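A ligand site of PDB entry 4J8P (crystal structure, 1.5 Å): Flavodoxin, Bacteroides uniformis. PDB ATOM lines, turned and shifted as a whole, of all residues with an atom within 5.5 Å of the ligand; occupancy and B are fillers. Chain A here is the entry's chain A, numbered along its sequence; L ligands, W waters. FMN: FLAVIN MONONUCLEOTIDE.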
ATOM      1  N   PHE A  13       2.213  27.554  13.926  1.00  0.00           N
ATOM      2  CA  PHE A  13       3.517  26.905  13.805  1.00  0.00           C
ATOM      3  C   PHE A  13       3.275  25.440  13.379  1.00  0.00           C
ATOM      4  O   PHE A  13       2.367  24.783  13.920  1.00  0.00           O
ATOM      5  CB  PHE A  13       4.304  26.969  15.138  1.00  0.00           C
ATOM      6  CG  PHE A  13       5.480  26.037  15.201  1.00  0.00           C
ATOM      7  CD1 PHE A  13       6.602  26.233  14.410  1.00  0.00           C
ATOM      8  CD2 PHE A  13       5.464  24.943  16.072  1.00  0.00           C
ATOM      9  CE1 PHE A  13       7.682  25.336  14.462  1.00  0.00           C
ATOM     10  CE2 PHE A  13       6.555  24.071  16.143  1.00  0.00           C
ATOM     11  CZ  PHE A  13       7.665  24.271  15.344  1.00  0.00           C
ATOM     12  N   SER A  14       4.108  24.921  12.439  1.00  0.00           N
ATOM     13  CA  SER A  14       3.934  23.536  12.028  1.00  0.00           C
ATOM     14  C   SER A  14       5.278  22.993  11.622  1.00  0.00           C
ATOM     15  O   SER A  14       5.951  23.617  10.793  1.00  0.00           O
ATOM     16  CB  SER A  14       2.936  23.469  10.870  1.00  0.00           C
ATOM     17  OG  SER A  14       2.691  22.138  10.429  1.00  0.00           O
ATOM     18  N   ALA A  15       5.687  21.875  12.196  1.00  0.00           N
ATOM     19  CA  ALA A  15       6.992  21.293  11.838  1.00  0.00           C
ATOM     20  C   ALA A  15       6.895  20.289  10.692  1.00  0.00           C
ATOM     21  O   ALA A  15       7.864  20.144   9.927  1.00  0.00           O
ATOM     22  CB  ALA A  15       7.622  20.608  13.058  1.00  0.00           C
ATOM     23  N   THR A  16       5.787  19.530  10.618  1.00  0.00           N
ATOM     24  CA  THR A  16       5.614  18.500   9.598  1.00  0.00           C
ATOM     25  C   THR A  16       4.290  18.674   8.818  1.00  0.00           C
ATOM     26  O   THR A  16       3.818  17.727   8.199  1.00  0.00           O
ATOM     27  CB  THR A  16       5.766  17.071  10.199  1.00  0.00           C
ATOM     28  OG1 THR A  16       4.951  16.883  11.373  1.00  0.00           O
ATOM     29  CG2 THR A  16       7.211  16.784  10.596  1.00  0.00           C
ATOM     30  N   GLY A  17       3.735  19.879   8.809  1.00  0.00           N
ATOM     31  CA  GLY A  17       2.608  20.213   7.948  1.00  0.00           C
ATOM     32  C   GLY A  17       1.195  19.899   8.388  1.00  0.00           C
ATOM     33  O   GLY A  17       0.249  20.352   7.727  1.00  0.00           O
ATOM     34  N   THR A  18       1.011  19.165   9.495  1.00  0.00           N
ATOM     35  CA  THR A  18      -0.337  18.808   9.938  1.00  0.00           C
ATOM     36  C   THR A  18      -1.111  20.048  10.403  1.00  0.00           C
ATOM     37  O   THR A  18      -2.224  20.317   9.917  1.00  0.00           O
ATOM     38  CB  THR A  18      -0.289  17.778  11.069  1.00  0.00           C
ATOM     39  OG1 THR A  18       0.576  16.716  10.672  1.00  0.00           O
ATOM     40  CG2 THR A  18      -1.675  17.249  11.402  1.00  0.00           C
ATOM     41  N   THR A  19      -0.493  20.838  11.302  1.00  0.00           N
ATOM     42  CA  THR A  19      -1.122  22.067  11.830  1.00  0.00           C
ATOM     43  C   THR A  19      -1.243  23.108  10.696  1.00  0.00           C
ATOM     44  O   THR A  19      -2.214  23.865  10.677  1.00  0.00           O
ATOM     45  CB  THR A  19      -0.310  22.596  13.003  1.00  0.00           C
ATOM     46  OG1 THR A  19      -0.101  21.532  13.945  1.00  0.00           O
ATOM     47  CG2 THR A  19      -1.018  23.723  13.717  1.00  0.00           C
ATOM     48  N   ALA A  20      -0.283  23.123   9.731  1.00  0.00           N
ATOM     49  CA  ALA A  20      -0.371  24.051   8.615  1.00  0.00           C
ATOM     50  C   ALA A  20      -1.669  23.846   7.819  1.00  0.00           C
ATOM     51  O   ALA A  20      -2.333  24.802   7.447  1.00  0.00           O
ATOM     52  CB  ALA A  20       0.838  23.850   7.690  1.00  0.00           C
ATOM     53  N   LEU A  48      13.216  16.795  16.099  1.00  0.00           N
ATOM     54  CA  LEU A  48      11.872  16.326  16.413  1.00  0.00           C
ATOM     55  C   LEU A  48      11.860  14.918  17.014  1.00  0.00           C
ATOM     56  O   LEU A  48      10.782  14.404  17.253  1.00  0.00           O
ATOM     57  CB  LEU A  48      11.018  16.366  15.144  1.00  0.00           C
ATOM     58  CG  LEU A  48      10.818  17.741  14.544  1.00  0.00           C
ATOM     59  CD1 LEU A  48      10.142  17.635  13.182  1.00  0.00           C
ATOM     60  CD2 LEU A  48       9.930  18.598  15.490  1.00  0.00           C
ATOM     61  N   TRP A  50      11.455  12.762  19.611  1.00  0.00           N
ATOM     62  CA  TRP A  50      10.891  12.816  20.972  1.00  0.00           C
ATOM     63  C   TRP A  50      11.555  11.780  21.903  1.00  0.00           C
ATOM     64  O   TRP A  50      11.556  11.946  23.118  1.00  0.00           O
ATOM     65  CB  TRP A  50       9.347  12.598  20.922  1.00  0.00           C
ATOM     66  CG  TRP A  50       9.032  11.271  20.324  1.00  0.00           C
ATOM     67  CD1 TRP A  50       8.968  10.966  18.994  1.00  0.00           C
ATOM     68  CD2 TRP A  50       8.995  10.019  21.021  1.00  0.00           C
ATOM     69  NE1 TRP A  50       8.930   9.600  18.822  1.00  0.00           N
ATOM     70  CE2 TRP A  50       8.953   8.993  20.050  1.00  0.00           C
ATOM     71  CE3 TRP A  50       9.056   9.659  22.387  1.00  0.00           C
ATOM     72  CZ2 TRP A  50       8.909   7.637  20.395  1.00  0.00           C
ATOM     73  CZ3 TRP A  50       9.019   8.317  22.724  1.00  0.00           C
ATOM     74  CH2 TRP A  50       8.962   7.319  21.735  1.00  0.00           C
ATOM     75  N   SER A  57      13.983  19.438  20.506  1.00  0.00           N
ATOM     76  CA  SER A  57      12.631  19.539  21.066  1.00  0.00           C
ATOM     77  C   SER A  57      12.593  19.027  22.495  1.00  0.00           C
ATOM     78  O   SER A  57      11.848  19.579  23.319  1.00  0.00           O
ATOM     79  CB  SER A  57      11.618  18.796  20.204  1.00  0.00           C
ATOM     80  OG  SER A  57      11.843  17.391  20.113  1.00  0.00           O
ATOM     81  N   MET A  61      11.392  21.553  25.457  1.00  0.00           N
ATOM     82  CA  MET A  61      10.180  21.225  26.197  1.00  0.00           C
ATOM     83  C   MET A  61      10.481  20.960  27.688  1.00  0.00           C
ATOM     84  O   MET A  61       9.555  21.046  28.498  1.00  0.00           O
ATOM     85  CB  MET A  61       9.376  20.102  25.530  1.00  0.00           C
ATOM     86  CG  MET A  61       8.933  20.448  24.078  1.00  0.00           C
ATOM     87  SD  MET A  61       8.187  22.268  23.903  1.00  0.00           S
ATOM     88  CE  MET A  61       6.718  22.151  25.104  1.00  0.00           C
ATOM     89  N   PRO A  88       1.235  22.284  16.906  1.00  0.00           N
ATOM     90  CA  PRO A  88       1.172  20.881  17.346  1.00  0.00           C
ATOM     91  C   PRO A  88       1.323  20.785  18.867  1.00  0.00           C
ATOM     92  O   PRO A  88       1.997  21.634  19.439  1.00  0.00           O
ATOM     93  CB  PRO A  88       2.385  20.248  16.695  1.00  0.00           C
ATOM     94  CG  PRO A  88       3.405  21.390  16.571  1.00  0.00           C
ATOM     95  CD  PRO A  88       2.569  22.655  16.341  1.00  0.00           C
ATOM     96  N   ILE A  89       0.745  19.767  19.497  1.00  0.00           N
ATOM     97  CA  ILE A  89       0.996  19.580  20.918  1.00  0.00           C
ATOM     98  C   ILE A  89       2.344  18.866  21.057  1.00  0.00           C
ATOM     99  O   ILE A  89       2.518  17.799  20.460  1.00  0.00           O
ATOM    100  CB  ILE A  89      -0.116  18.722  21.538  1.00  0.00           C
ATOM    101  CG1 ILE A  89      -1.477  19.435  21.488  1.00  0.00           C
ATOM    102  CG2 ILE A  89       0.251  18.292  22.986  1.00  0.00           C
ATOM    103  CD1 ILE A  89      -1.579  20.704  22.232  1.00  0.00           C
ATOM    104  N   TRP A  90       3.263  19.444  21.845  1.00  0.00           N
ATOM    105  CA  TRP A  90       4.545  18.804  22.157  1.00  0.00           C
ATOM    106  C   TRP A  90       4.580  18.568  23.651  1.00  0.00           C
ATOM    107  O   TRP A  90       4.573  19.531  24.445  1.00  0.00           O
ATOM    108  CB  TRP A  90       5.709  19.685  21.708  1.00  0.00           C
ATOM    109  CG  TRP A  90       5.969  19.707  20.223  1.00  0.00           C
ATOM    110  CD1 TRP A  90       5.233  19.125  19.220  1.00  0.00           C
ATOM    111  CD2 TRP A  90       7.061  20.381  19.583  1.00  0.00           C
ATOM    112  NE1 TRP A  90       5.828  19.376  17.986  1.00  0.00           N
ATOM    113  CE2 TRP A  90       6.950  20.141  18.190  1.00  0.00           C
ATOM    114  CE3 TRP A  90       8.132  21.159  20.064  1.00  0.00           C
ATOM    115  CZ2 TRP A  90       7.835  20.723  17.278  1.00  0.00           C
ATOM    116  CZ3 TRP A  90       9.033  21.694  19.163  1.00  0.00           C
ATOM    117  CH2 TRP A  90       8.895  21.458  17.789  1.00  0.00           C
ATOM    118  N   TRP A  91       4.629  17.293  24.037  1.00  0.00           N
ATOM    119  CA  TRP A  91       4.668  16.964  25.463  1.00  0.00           C
ATOM    120  C   TRP A  91       3.576  17.733  26.269  1.00  0.00           C
ATOM    121  O   TRP A  91       3.853  18.321  27.331  1.00  0.00           O
ATOM    122  CB  TRP A  91       6.065  17.160  26.082  1.00  0.00           C
ATOM    123  CG  TRP A  91       7.105  16.276  25.441  1.00  0.00           C
ATOM    124  CD1 TRP A  91       8.086  16.659  24.576  1.00  0.00           C
ATOM    125  CD2 TRP A  91       7.158  14.833  25.504  1.00  0.00           C
ATOM    126  NE1 TRP A  91       8.832  15.563  24.181  1.00  0.00           N
ATOM    127  CE2 TRP A  91       8.265  14.433  24.712  1.00  0.00           C
ATOM    128  CE3 TRP A  91       6.403  13.858  26.187  1.00  0.00           C
ATOM    129  CZ2 TRP A  91       8.642  13.084  24.587  1.00  0.00           C
ATOM    130  CZ3 TRP A  91       6.788  12.523  26.054  1.00  0.00           C
ATOM    131  CH2 TRP A  91       7.869  12.159  25.249  1.00  0.00           C
ATOM    132  N   ASN A  92       2.325  17.690  25.730  1.00  0.00           N
ATOM    133  CA  ASN A  92       1.156  18.255  26.422  1.00  0.00           C
ATOM    134  C   ASN A  92       1.234  19.788  26.550  1.00  0.00           C
ATOM    135  O   ASN A  92       0.481  20.381  27.347  1.00  0.00           O
ATOM    136  CB  ASN A  92       1.030  17.624  27.826  1.00  0.00           C
ATOM    137  CG  ASN A  92      -0.356  17.697  28.405  1.00  0.00           C
ATOM    138  OD1 ASN A  92      -1.358  17.846  27.698  1.00  0.00           O
ATOM    139  ND2 ASN A  92      -0.451  17.614  29.712  1.00  0.00           N
ATOM    140  N   LEU A  93       2.078  20.446  25.718  1.00  0.00           N
ATOM    141  CA  LEU A  93       2.255  21.883  25.789  1.00  0.00           C
ATOM    142  C   LEU A  93       2.304  22.477  24.398  1.00  0.00           C
ATOM    143  O   LEU A  93       2.530  21.778  23.415  1.00  0.00           O
ATOM    144  CB  LEU A  93       3.588  22.195  26.497  1.00  0.00           C
ATOM    145  CG  LEU A  93       3.641  21.899  28.008  1.00  0.00           C
ATOM    146  CD1 LEU A  93       5.089  21.799  28.506  1.00  0.00           C
ATOM    147  CD2 LEU A  93       2.888  22.969  28.787  1.00  0.00           C
ATOM    148  N   THR A 117      -3.095  20.451  16.839  1.00  0.00           N
ATOM    149  CA  THR A 117      -3.212  19.083  16.357  1.00  0.00           C
ATOM    150  C   THR A 117      -2.316  18.227  17.238  1.00  0.00           C
ATOM    151  O   THR A 117      -1.366  18.758  17.839  1.00  0.00           O
ATOM    152  CB  THR A 117      -2.861  18.950  14.860  1.00  0.00           C
ATOM    153  OG1 THR A 117      -1.462  19.157  14.677  1.00  0.00           O
ATOM    154  CG2 THR A 117      -3.683  19.921  13.984  1.00  0.00           C
ATOM    155  N   SER A 118      -2.641  16.949  17.368  1.00  0.00           N
ATOM    156  CA  SER A 118      -1.857  16.073  18.244  1.00  0.00           C
ATOM    157  C   SER A 118      -1.950  14.635  17.807  1.00  0.00           C
ATOM    158  O   SER A 118      -2.834  14.278  17.028  1.00  0.00           O
ATOM    159  CB  SER A 118      -2.382  16.178  19.671  1.00  0.00           C
ATOM    160  OG  SER A 118      -3.690  15.613  19.756  1.00  0.00           O
ATOM    161  N   GLY A 119      -1.084  13.781  18.368  1.00  0.00           N
ATOM    162  CA  GLY A 119      -1.196  12.345  18.153  1.00  0.00           C
ATOM    163  C   GLY A 119      -2.463  11.817  18.799  1.00  0.00           C
ATOM    164  O   GLY A 119      -3.184  11.007  18.208  1.00  0.00           O
ATOM    165  N   SER A 120      -2.779  12.306  20.029  1.00  0.00           N
ATOM    166  CA  SER A 120      -3.980  11.947  20.766  1.00  0.00           C
ATOM    167  C   SER A 120      -4.314  12.879  21.924  1.00  0.00           C
ATOM    168  O   SER A 120      -5.475  12.949  22.344  1.00  0.00           O
ATOM    169  CB  SER A 120      -3.869  10.527  21.314  1.00  0.00           C
ATOM    170  OG  SER A 120      -2.822  10.403  22.270  1.00  0.00           O
ATOM    171  N   SER A 121      -3.307  13.590  22.470  1.00  0.00           N
ATOM    172  CA  SER A 121      -3.558  14.419  23.649  1.00  0.00           C
ATOM    173  C   SER A 121      -4.544  15.538  23.375  1.00  0.00           C
ATOM    174  O   SER A 121      -4.655  16.065  22.245  1.00  0.00           O
ATOM    175  CB  SER A 121      -2.261  15.058  24.138  1.00  0.00           C
ATOM    176  OG  SER A 121      -1.305  14.068  24.521  1.00  0.00           O
ATOM    177  N   ASN A 146      -7.935  17.578  15.202  1.00  0.00           N
ATOM    178  CA  ASN A 146      -7.330  16.381  14.616  1.00  0.00           C
ATOM    179  C   ASN A 146      -8.190  15.892  13.478  1.00  0.00           C
ATOM    180  O   ASN A 146      -9.401  16.091  13.521  1.00  0.00           O
ATOM    181  CB  ASN A 146      -7.117  15.293  15.678  1.00  0.00           C
ATOM    182  CG  ASN A 146      -5.901  15.607  16.521  1.00  0.00           C
ATOM    183  OD1 ASN A 146      -5.030  16.371  16.093  1.00  0.00           O
ATOM    184  ND2 ASN A 146      -5.783  14.986  17.702  1.00  0.00           N
HETATM  185  N1  FMN L   1       1.169  14.286  20.352  1.00  0.00           N
HETATM  186  C2  FMN L   1       0.395  14.078  21.467  1.00  0.00           C
HETATM  187  O2  FMN L   1      -0.719  13.539  21.400  1.00  0.00           O
HETATM  188  N3  FMN L   1       0.893  14.419  22.737  1.00  0.00           N
HETATM  189  C4  FMN L   1       2.158  14.919  22.996  1.00  0.00           C
HETATM  190  O4  FMN L   1       2.463  15.239  24.148  1.00  0.00           O
HETATM  191  C4A FMN L   1       3.008  15.046  21.814  1.00  0.00           C
HETATM  192  N5  FMN L   1       4.270  15.384  21.992  1.00  0.00           N
HETATM  193  C5A FMN L   1       5.078  15.513  20.863  1.00  0.00           C
HETATM  194  C6  FMN L   1       6.405  15.928  21.034  1.00  0.00           C
HETATM  195  C7  FMN L   1       7.232  16.171  19.943  1.00  0.00           C
HETATM  196  C7M FMN L   1       8.598  16.755  20.178  1.00  0.00           C
HETATM  197  C8  FMN L   1       6.738  15.949  18.639  1.00  0.00           C
HETATM  198  C8M FMN L   1       7.569  16.256  17.430  1.00  0.00           C
HETATM  199  C9  FMN L   1       5.436  15.509  18.476  1.00  0.00           C
HETATM  200  C9A FMN L   1       4.585  15.290  19.559  1.00  0.00           C
HETATM  201  N10 FMN L   1       3.223  14.883  19.421  1.00  0.00           N
HETATM  202  C10 FMN L   1       2.421  14.735  20.519  1.00  0.00           C
HETATM  203  C1' FMN L   1       2.688  14.661  18.061  1.00  0.00           C
HETATM  204  C2' FMN L   1       2.235  15.948  17.375  1.00  0.00           C
HETATM  205  O2' FMN L   1       1.473  16.786  18.232  1.00  0.00           O
HETATM  206  C3' FMN L   1       1.404  15.698  16.112  1.00  0.00           C
HETATM  207  O3' FMN L   1       2.053  14.704  15.298  1.00  0.00           O
HETATM  208  C4' FMN L   1       1.136  16.989  15.333  1.00  0.00           C
HETATM  209  O4' FMN L   1      -0.030  16.788  14.531  1.00  0.00           O
HETATM  210  C5' FMN L   1       2.320  17.340  14.444  1.00  0.00           C
HETATM  211  O5' FMN L   1       1.976  18.597  13.842  1.00  0.00           O
HETATM  212  P   FMN L   1       2.838  19.355  12.772  1.00  0.00           P
HETATM  213  O1P FMN L   1       4.195  19.723  13.245  1.00  0.00           O
HETATM  214  O2P FMN L   1       1.987  20.544  12.429  1.00  0.00           O
HETATM  215  O3P FMN L   1       2.901  18.440  11.536  1.00  0.00           O
HETATM  216  O   HOH W   1      11.084  15.882  22.341  1.00  0.00           O
HETATM  217  O   HOH W   2      -2.809  15.093  14.299  1.00  0.00           O
HETATM  218  O   HOH W   3       5.428  18.478  15.378  1.00  0.00           O
HETATM  219  O   HOH W   4       4.761  14.491  15.066  1.00  0.00           O
HETATM  220  O   HOH W   5       1.345  12.163  15.858  1.00  0.00           O
HETATM  221  O   HOH W   6       0.590  14.576  12.520  1.00  0.00           O
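N of Thr 16 is in hydrogen-bond range of O1P of the ligand, at 3.1 Å.
The side-chain hydroxyl (OG1) of Thr 16 lies within hydrogen-bond range of an oxygen (O3P) of the ligand, at 2.6 Å.
An oxygen (O2P) of the ligand lies within hydrogen-bond range of the side-chain hydroxyl (OG) of Ser 14, 2.7 Å away.
An oxygen (O2') of the ligand lies within hydrogen-bond range of the backbone NH (N) of Ile 89 (3.3 Å).
O of Ile 89 is in hydrogen-bond range of O2' of the ligand, 2.7 Å away.
N of Thr 19 sits at hydrogen-bond distance from O2P of the ligand, 2.7 Å away.
The side-chain hydroxyl of Thr 19 lies within hydrogen-bond range of an oxygen (O2P) of the ligand.
O2 of the ligand is in hydrogen-bond range of N of Ser 120 (2.8 Å).
The backbone carbonyl oxygen (O) of Thr 117 lies within hydrogen-bond range of an oxygen (O2') of the ligand.
An oxygen (O4') of the ligand is in hydrogen-bond range of the side-chain hydroxyl of Thr 117, at 2.8 Å.
The backbone NH (N) of Ser 121 lies within hydrogen-bond range of an oxygen (O2) of the ligand, at 2.8 Å.
N3 of the ligand sits at hydrogen-bond distance from OG of Ser 121.
A nitrogen (N5) of the ligand lies within hydrogen-bond range of the backbone NH of Trp 91, 2.8 Å away.
The backbone NH of Ala 15 lies within hydrogen-bond range of an oxygen (O1P) of the ligand, at 2.8 Å.
The backbone NH of Thr 18 lies within hydrogen-bond range of an oxygen (O3P) of the ligand (2.9 Å).
The side-chain hydroxyl (OG1) of Thr 18 is in hydrogen-bond range of an oxygen (O3P) of the ligand, at 3.0 Å.
N of Asn 92 is in hydrogen-bond range of O4 of the ligand, 2.9 Å away.
A nitrogen (N1) of the ligand sits at hydrogen-bond distance from the backbone NH (N) of Gly 119.
An oxygen (O3P) of the ligand sits at hydrogen-bond distance from the backbone NH (N) of Gly 17, 3.2 Å away.
The side-chain hydroxyl (OG) of Ser 14 is in hydrogen-bond range of the backbone NH (N) of Gly 17 (3.0 Å).
The side-chain hydroxyl of Ser 14 sits at hydrogen-bond distance from the backbone NH of Ala 20.
The backbone NH of Ile 89 lies within hydrogen-bond range of the backbone carbonyl oxygen of Thr 117 (2.9 Å).
The side-chain hydroxyl (OG1) of Thr 19 sits at hydrogen-bond distance from the side-chain hydroxyl (OG1) of Thr 117, 2.8 Å away.
OG of Ser 118 sits close to N of Ser 120 (3.4 Å).
OG of Ser 118 is in hydrogen-bond range of O of Ser 121 (2.7 Å).
N of Ser 118 lies within hydrogen-bond range of OD1 of Asn 146 (2.8 Å).
Residues that only touch the ligand: Ser 57, Pro 88, Ser 118, Trp 90 and Leu 48.
Hydrophobic or aromatic side chains that line the ligand: Ala 15, Leu 48, Pro 88, Ile 89, Trp 90 and Trp 91.
Water W3 bridges an oxygen (O1P) of the ligand (2.8 Å) and the indole nitrogen (NE1) of Trp 90 (2.8 Å).
Water W6 bridges the side-chain hydroxyl (OG1) of Thr 18 and an oxygen (O4') of the ligand.
Water W2 lies within hydrogen-bond range of O of Ser 118, OD1 of Asn 146 and O4' of the ligand.
Water W1 bridges OG of Ser 57 (2.8 Å) and NE1 of Trp 91 (2.9 Å).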
